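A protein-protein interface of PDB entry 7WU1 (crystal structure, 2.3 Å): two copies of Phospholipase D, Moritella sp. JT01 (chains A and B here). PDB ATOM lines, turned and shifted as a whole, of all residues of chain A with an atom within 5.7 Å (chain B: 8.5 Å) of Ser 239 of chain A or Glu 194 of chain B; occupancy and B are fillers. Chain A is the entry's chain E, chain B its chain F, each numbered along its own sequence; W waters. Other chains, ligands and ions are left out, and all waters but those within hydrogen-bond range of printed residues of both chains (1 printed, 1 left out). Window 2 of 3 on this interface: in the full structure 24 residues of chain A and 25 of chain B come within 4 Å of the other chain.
Leu 237 of chain A touches its own counterpart, Leu 237 of chain B.
Of the 6 pairs that touch across the chains among the printed residues, 1 has its exchanged pair printed and touching as well.
Water W1 bridges the backbone NH (N) of Ala 193 of chain B (2.5 Å) and the backbone carbonyl oxygen (O) of Leu 237 of chain A (3.3 Å).
Hydrophobic or aromatic side chains of chain A within 4 Å of the printed part of chain B: Leu 237 and Ile 238.
Of the 14 printed residues of chain B, 4 touch a printed residue of chain A.
Hydrophobic or aromatic side chains of chain B within 4 Å of the printed part of chain A: Ala 193.
SG of Cys 241 of chain A forms a disulfide with SG of Cys 234 of chain A.
O of Ser 239 of chain A sits close to OD1 of Asn 253 of chain A, 3.3 Å away.
The backbone carbonyl oxygen (O) of Asn 253 of chain A lies within hydrogen-bond range of the backbone NH (N) of Leu 237 of chain A, at 2.9 Å.
The backbone carbonyl oxygen (O) of Ile 238 of chain A lies within hydrogen-bond range of the backbone NH (N) of Glu 194 of chain B, at 3.4 Å.
ND2 of Asn 253 of chain A sits at hydrogen-bond distance from OD1 of Asp 192 of chain B.
Among the printed residues, merely in contact across the chains: Leu 237 of chain A with Leu 237 of chain B (3.99 Å), Ile 238 of chain A with Asp 192 of chain B (3.3 Å), Ile 238 of chain A with Ala 193 of chain B (3.6 Å) and Ser 239 of chain A with Glu 194 of chain B (3.5 Å).
Of chain B, only Glu 194 comes within 4 Å of Ser 239 of chain A.
Of the printed residues of chain A, Glu 194 of chain B touches Ile 238 and Ser 239.
Of the printed residues of chain B, Leu 237 of chain A touches Leu 237 (3.99 Å).
Printed residues of chain B within 4 Å of Ile 238 of chain A: Asp 192, Ala 193 and Glu 194.
Of the printed residues of chain A, Asp 192 of chain B touches Ile 238 and Asn 253.
Of the printed residues of chain B, Asn 253 of chain A touches Asp 192.
Asn 235 of chain B touches none of the printed residues of chain A.
The nearest residue of chain B that does not touch Ser 239 of chain A is Asp 192 of chain B (4.1 Å).
The nearest printed residue of chain B that does not touch Asn 253 of chain A is Ala 193 of chain B (5.8 Å).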
ATOM      1  N   CYS A 234       7.431  17.460   4.142  1.00  0.00           N
ATOM      2  CA  CYS A 234       7.508  18.008   2.794  1.00  0.00           C
ATOM      3  C   CYS A 234       8.965  18.124   2.381  1.00  0.00           C
ATOM      4  O   CYS A 234       9.803  18.591   3.154  1.00  0.00           O
ATOM      5  CB  CYS A 234       6.802  19.343   2.743  1.00  0.00           C
ATOM      6  SG  CYS A 234       6.866  20.230   1.170  1.00  0.00           S
ATOM      7  N   LYS A 236       9.543  18.899  -1.200  1.00  0.00           N
ATOM      8  CA  LYS A 236       9.327  19.207  -2.613  1.00  0.00           C
ATOM      9  C   LYS A 236      10.399  20.137  -3.170  1.00  0.00           C
ATOM     10  O   LYS A 236      10.937  19.884  -4.252  1.00  0.00           O
ATOM     11  CB  LYS A 236       7.931  19.817  -2.792  1.00  0.00           C
ATOM     12  CG  LYS A 236       6.806  18.797  -2.742  1.00  0.00           C
ATOM     13  CD  LYS A 236       5.438  19.464  -2.780  1.00  0.00           C
ATOM     14  CE  LYS A 236       4.354  18.483  -2.339  1.00  0.00           C
ATOM     15  NZ  LYS A 236       2.987  19.084  -2.392  1.00  0.00           N
ATOM     16  N   LEU A 237      10.686  21.244  -2.461  1.00  0.00           N
ATOM     17  CA  LEU A 237      11.606  22.285  -2.905  1.00  0.00           C
ATOM     18  C   LEU A 237      11.008  23.154  -4.009  1.00  0.00           C
ATOM     19  O   LEU A 237      11.174  24.389  -3.991  1.00  0.00           O
ATOM     20  CB  LEU A 237      12.917  21.682  -3.402  1.00  0.00           C
ATOM     21  CG  LEU A 237      13.844  21.112  -2.336  1.00  0.00           C
ATOM     22  CD1 LEU A 237      15.003  20.363  -2.961  1.00  0.00           C
ATOM     23  CD2 LEU A 237      14.341  22.220  -1.376  1.00  0.00           C
ATOM     24  N   ILE A 238      10.290  22.528  -4.951  1.00  0.00           N
ATOM     25  CA  ILE A 238       9.831  23.210  -6.162  1.00  0.00           C
ATOM     26  C   ILE A 238       8.388  23.686  -6.072  1.00  0.00           C
ATOM     27  O   ILE A 238       7.877  24.251  -7.045  1.00  0.00           O
ATOM     28  CB  ILE A 238       9.987  22.318  -7.413  1.00  0.00           C
ATOM     29  CG1 ILE A 238       8.921  21.216  -7.379  1.00  0.00           C
ATOM     30  CG2 ILE A 238      11.393  21.731  -7.491  1.00  0.00           C
ATOM     31  CD1 ILE A 238       9.196  20.024  -8.318  1.00  0.00           C
ATOM     32  N   SER A 239       7.710  23.467  -4.951  1.00  0.00           N
ATOM     33  CA  SER A 239       6.295  23.808  -4.878  1.00  0.00           C
ATOM     34  C   SER A 239       5.869  23.894  -3.415  1.00  0.00           C
ATOM     35  O   SER A 239       6.601  23.506  -2.499  1.00  0.00           O
ATOM     36  CB  SER A 239       5.441  22.795  -5.663  1.00  0.00           C
ATOM     37  OG  SER A 239       5.132  21.659  -4.898  1.00  0.00           O
ATOM     38  N   ASN A 240       4.664  24.424  -3.219  1.00  0.00           N
ATOM     39  CA  ASN A 240       4.182  24.753  -1.883  1.00  0.00           C
ATOM     40  C   ASN A 240       4.012  23.511  -1.018  1.00  0.00           C
ATOM     41  O   ASN A 240       3.552  22.468  -1.479  1.00  0.00           O
ATOM     42  CB  ASN A 240       2.848  25.496  -1.988  1.00  0.00           C
ATOM     43  CG  ASN A 240       2.406  26.089  -0.680  1.00  0.00           C
ATOM     44  OD1 ASN A 240       1.624  25.482   0.050  1.00  0.00           O
ATOM     45  ND2 ASN A 240       2.912  27.300  -0.364  1.00  0.00           N
ATOM     46  N   CYS A 241       4.358  23.637   0.253  1.00  0.00           N
ATOM     47  CA  CYS A 241       4.261  22.528   1.190  1.00  0.00           C
ATOM     48  C   CYS A 241       2.869  22.373   1.802  1.00  0.00           C
ATOM     49  O   CYS A 241       2.592  21.349   2.436  1.00  0.00           O
ATOM     50  CB  CYS A 241       5.290  22.714   2.311  1.00  0.00           C
ATOM     51  SG  CYS A 241       6.977  22.286   1.877  1.00  0.00           S
ATOM     52  N   ASN A 253       9.911  25.632   0.976  1.00  0.00           N
ATOM     53  CA  ASN A 253       9.273  24.473   0.365  1.00  0.00           C
ATOM     54  C   ASN A 253       9.831  23.141   0.876  1.00  0.00           C
ATOM     55  O   ASN A 253       9.852  22.134   0.146  1.00  0.00           O
ATOM     56  CB  ASN A 253       9.398  24.575  -1.154  1.00  0.00           C
ATOM     57  CG  ASN A 253       8.589  25.719  -1.725  1.00  0.00           C
ATOM     58  OD1 ASN A 253       7.722  26.270  -1.057  1.00  0.00           O
ATOM     59  ND2 ASN A 253       8.868  26.078  -2.959  1.00  0.00           N
ATOM     60  N   THR B 186      16.946  31.591 -11.147  1.00  0.00           N
ATOM     61  CA  THR B 186      15.838  30.643 -11.354  1.00  0.00           C
ATOM     62  C   THR B 186      15.831  29.665 -10.191  1.00  0.00           C
ATOM     63  O   THR B 186      16.878  29.090  -9.876  1.00  0.00           O
ATOM     64  CB  THR B 186      15.966  29.871 -12.680  1.00  0.00           C
ATOM     65  OG1 THR B 186      14.783  29.092 -12.893  1.00  0.00           O
ATOM     66  CG2 THR B 186      17.163  28.909 -12.697  1.00  0.00           C
ATOM     67  N   PRO B 187      14.685  29.433  -9.546  1.00  0.00           N
ATOM     68  CA  PRO B 187      13.394  30.107  -9.791  1.00  0.00           C
ATOM     69  C   PRO B 187      13.422  31.589  -9.482  1.00  0.00           C
ATOM     70  O   PRO B 187      14.151  32.036  -8.594  1.00  0.00           O
ATOM     71  CB  PRO B 187      12.414  29.386  -8.847  1.00  0.00           C
ATOM     72  CG  PRO B 187      13.304  28.664  -7.833  1.00  0.00           C
ATOM     73  CD  PRO B 187      14.564  28.307  -8.602  1.00  0.00           C
ATOM     74  N   MET B 188      12.624  32.338 -10.232  1.00  0.00           N
ATOM     75  CA  MET B 188      12.611  33.791 -10.153  1.00  0.00           C
ATOM     76  C   MET B 188      11.725  34.272  -9.013  1.00  0.00           C
ATOM     77  O   MET B 188      10.760  33.600  -8.616  1.00  0.00           O
ATOM     78  CB  MET B 188      12.134  34.359 -11.489  1.00  0.00           C
ATOM     79  CG  MET B 188      11.599  35.790 -11.476  1.00  0.00           C
ATOM     80  SD  MET B 188      11.026  36.335 -13.154  1.00  0.00           S
ATOM     81  CE  MET B 188      12.238  35.524 -14.216  1.00  0.00           C
ATOM     82  N   TYR B 191       7.977  33.189  -7.994  1.00  0.00           N
ATOM     83  CA  TYR B 191       7.583  31.982  -8.704  1.00  0.00           C
ATOM     84  C   TYR B 191       8.275  30.769  -8.106  1.00  0.00           C
ATOM     85  O   TYR B 191       9.488  30.793  -7.887  1.00  0.00           O
ATOM     86  CB  TYR B 191       7.934  32.087 -10.197  1.00  0.00           C
ATOM     87  CG  TYR B 191       7.280  33.258 -10.885  1.00  0.00           C
ATOM     88  CD1 TYR B 191       6.020  33.123 -11.478  1.00  0.00           C
ATOM     89  CD2 TYR B 191       7.911  34.500 -10.929  1.00  0.00           C
ATOM     90  CE1 TYR B 191       5.406  34.193 -12.105  1.00  0.00           C
ATOM     91  CE2 TYR B 191       7.314  35.568 -11.550  1.00  0.00           C
ATOM     92  CZ  TYR B 191       6.054  35.415 -12.137  1.00  0.00           C
ATOM     93  OH  TYR B 191       5.438  36.483 -12.754  1.00  0.00           O
ATOM     94  N   ASP B 192       7.501  29.728  -7.826  1.00  0.00           N
ATOM     95  CA  ASP B 192       8.082  28.429  -7.539  1.00  0.00           C
ATOM     96  C   ASP B 192       8.741  27.859  -8.800  1.00  0.00           C
ATOM     97  O   ASP B 192       8.399  28.210  -9.940  1.00  0.00           O
ATOM     98  CB  ASP B 192       7.013  27.471  -7.007  1.00  0.00           C
ATOM     99  CG  ASP B 192       6.502  27.875  -5.627  1.00  0.00           C
ATOM    100  OD1 ASP B 192       7.327  28.300  -4.790  1.00  0.00           O
ATOM    101  OD2 ASP B 192       5.277  27.759  -5.379  1.00  0.00           O
ATOM    102  N   ALA B 193       9.710  26.967  -8.584  1.00  0.00           N
ATOM    103  CA  ALA B 193      10.434  26.391  -9.711  1.00  0.00           C
ATOM    104  C   ALA B 193       9.517  25.664 -10.688  1.00  0.00           C
ATOM    105  O   ALA B 193       9.875  25.515 -11.863  1.00  0.00           O
ATOM    106  CB  ALA B 193      11.510  25.426  -9.211  1.00  0.00           C
ATOM    107  N   GLU B 194       8.342  25.211 -10.238  1.00  0.00           N
ATOM    108  CA  GLU B 194       7.425  24.501 -11.123  1.00  0.00           C
ATOM    109  C   GLU B 194       6.825  25.391 -12.208  1.00  0.00           C
ATOM    110  O   GLU B 194       6.230  24.862 -13.154  1.00  0.00           O
ATOM    111  CB  GLU B 194       6.302  23.862 -10.299  1.00  0.00           C
ATOM    112  CG  GLU B 194       5.374  24.860  -9.602  1.00  0.00           C
ATOM    113  CD  GLU B 194       4.268  24.168  -8.797  1.00  0.00           C
ATOM    114  OE1 GLU B 194       4.094  22.925  -8.927  1.00  0.00           O
ATOM    115  OE2 GLU B 194       3.566  24.866  -8.032  1.00  0.00           O
ATOM    116  N   SER B 195       6.992  26.708 -12.114  1.00  0.00           N
ATOM    117  CA  SER B 195       6.339  27.651 -13.023  1.00  0.00           C
ATOM    118  C   SER B 195       7.341  28.231 -14.020  1.00  0.00           C
ATOM    119  O   SER B 195       7.504  29.452 -14.139  1.00  0.00           O
ATOM    120  CB  SER B 195       5.657  28.771 -12.221  1.00  0.00           C
ATOM    121  OG  SER B 195       4.865  28.249 -11.158  1.00  0.00           O
ATOM    122  N   GLU B 196       7.997  27.342 -14.772  1.00  0.00           N
ATOM    123  CA  GLU B 196       8.970  27.787 -15.766  1.00  0.00           C
ATOM    124  C   GLU B 196       8.321  28.690 -16.818  1.00  0.00           C
ATOM    125  O   GLU B 196       8.877  29.732 -17.185  1.00  0.00           O
ATOM    126  CB  GLU B 196       9.626  26.582 -16.442  1.00  0.00           C
ATOM    127  CG  GLU B 196      10.336  25.612 -15.511  1.00  0.00           C
ATOM    128  CD  GLU B 196      10.454  24.189 -16.118  1.00  0.00           C
ATOM    129  OE1 GLU B 196       9.560  23.774 -16.914  1.00  0.00           O
ATOM    130  OE2 GLU B 196      11.436  23.469 -15.794  1.00  0.00           O
ATOM    131  N   GLU B 197       7.143  28.301 -17.314  1.00  0.00           N
ATOM    132  CA  GLU B 197       6.492  29.045 -18.391  1.00  0.00           C
ATOM    133  C   GLU B 197       6.276  30.508 -18.023  1.00  0.00           C
ATOM    134  O   GLU B 197       6.647  31.410 -18.793  1.00  0.00           O
ATOM    135  CB  GLU B 197       5.157  28.380 -18.720  1.00  0.00           C
ATOM    136  CG  GLU B 197       4.569  28.682 -20.109  1.00  0.00           C
ATOM    137  CD  GLU B 197       3.741  29.985 -20.134  1.00  0.00           C
ATOM    138  OE1 GLU B 197       3.104  30.325 -19.104  1.00  0.00           O
ATOM    139  OE2 GLU B 197       3.736  30.678 -21.185  1.00  0.00           O
ATOM    140  N   GLU B 198       5.623  30.767 -16.885  1.00  0.00           N
ATOM    141  CA  GLU B 198       5.411  32.148 -16.449  1.00  0.00           C
ATOM    142  C   GLU B 198       6.733  32.896 -16.305  1.00  0.00           C
ATOM    143  O   GLU B 198       6.823  34.095 -16.613  1.00  0.00           O
ATOM    144  CB  GLU B 198       4.651  32.161 -15.127  1.00  0.00           C
ATOM    145  CG  GLU B 198       3.200  31.701 -15.222  1.00  0.00           C
ATOM    146  CD  GLU B 198       2.957  30.314 -14.620  1.00  0.00           C
ATOM    147  OE1 GLU B 198       3.741  29.380 -14.925  1.00  0.00           O
ATOM    148  OE2 GLU B 198       1.975  30.150 -13.849  1.00  0.00           O
ATOM    149  N   GLU B 199       7.769  32.201 -15.832  1.00  0.00           N
ATOM    150  CA  GLU B 199       9.090  32.805 -15.694  1.00  0.00           C
ATOM    151  C   GLU B 199       9.606  33.314 -17.034  1.00  0.00           C
ATOM    152  O   GLU B 199      10.060  34.461 -17.145  1.00  0.00           O
ATOM    153  CB  GLU B 199      10.035  31.763 -15.092  1.00  0.00           C
ATOM    154  CG  GLU B 199      11.323  32.298 -14.533  1.00  0.00           C
ATOM    155  CD  GLU B 199      12.034  31.292 -13.640  1.00  0.00           C
ATOM    156  OE1 GLU B 199      11.415  30.813 -12.669  1.00  0.00           O
ATOM    157  OE2 GLU B 199      13.216  31.000 -13.908  1.00  0.00           O
ATOM    158  N   ASN B 235      18.051  24.488 -13.266  1.00  0.00           N
ATOM    159  CA  ASN B 235      17.025  24.812 -12.287  1.00  0.00           C
ATOM    160  C   ASN B 235      16.566  23.563 -11.541  1.00  0.00           C
ATOM    161  O   ASN B 235      15.439  23.507 -11.044  1.00  0.00           O
ATOM    162  CB  ASN B 235      15.835  25.485 -12.965  1.00  0.00           C
ATOM    163  CG  ASN B 235      15.054  24.527 -13.853  1.00  0.00           C
ATOM    164  OD1 ASN B 235      15.563  23.486 -14.269  1.00  0.00           O
ATOM    165  ND2 ASN B 235      13.807  24.876 -14.144  1.00  0.00           N
ATOM    166  N   LEU B 237      17.575  21.906  -8.629  1.00  0.00           N
ATOM    167  CA  LEU B 237      17.432  21.992  -7.183  1.00  0.00           C
ATOM    168  C   LEU B 237      17.579  20.654  -6.463  1.00  0.00           C
ATOM    169  O   LEU B 237      18.168  20.584  -5.375  1.00  0.00           O
ATOM    170  CB  LEU B 237      16.071  22.587  -6.826  1.00  0.00           C
ATOM    171  CG  LEU B 237      15.856  24.078  -7.089  1.00  0.00           C
ATOM    172  CD1 LEU B 237      14.355  24.422  -6.975  1.00  0.00           C
ATOM    173  CD2 LEU B 237      16.675  24.926  -6.160  1.00  0.00           C
HETATM  174  O   HOH W   1      10.676  26.696  -6.343  1.00  0.00           O
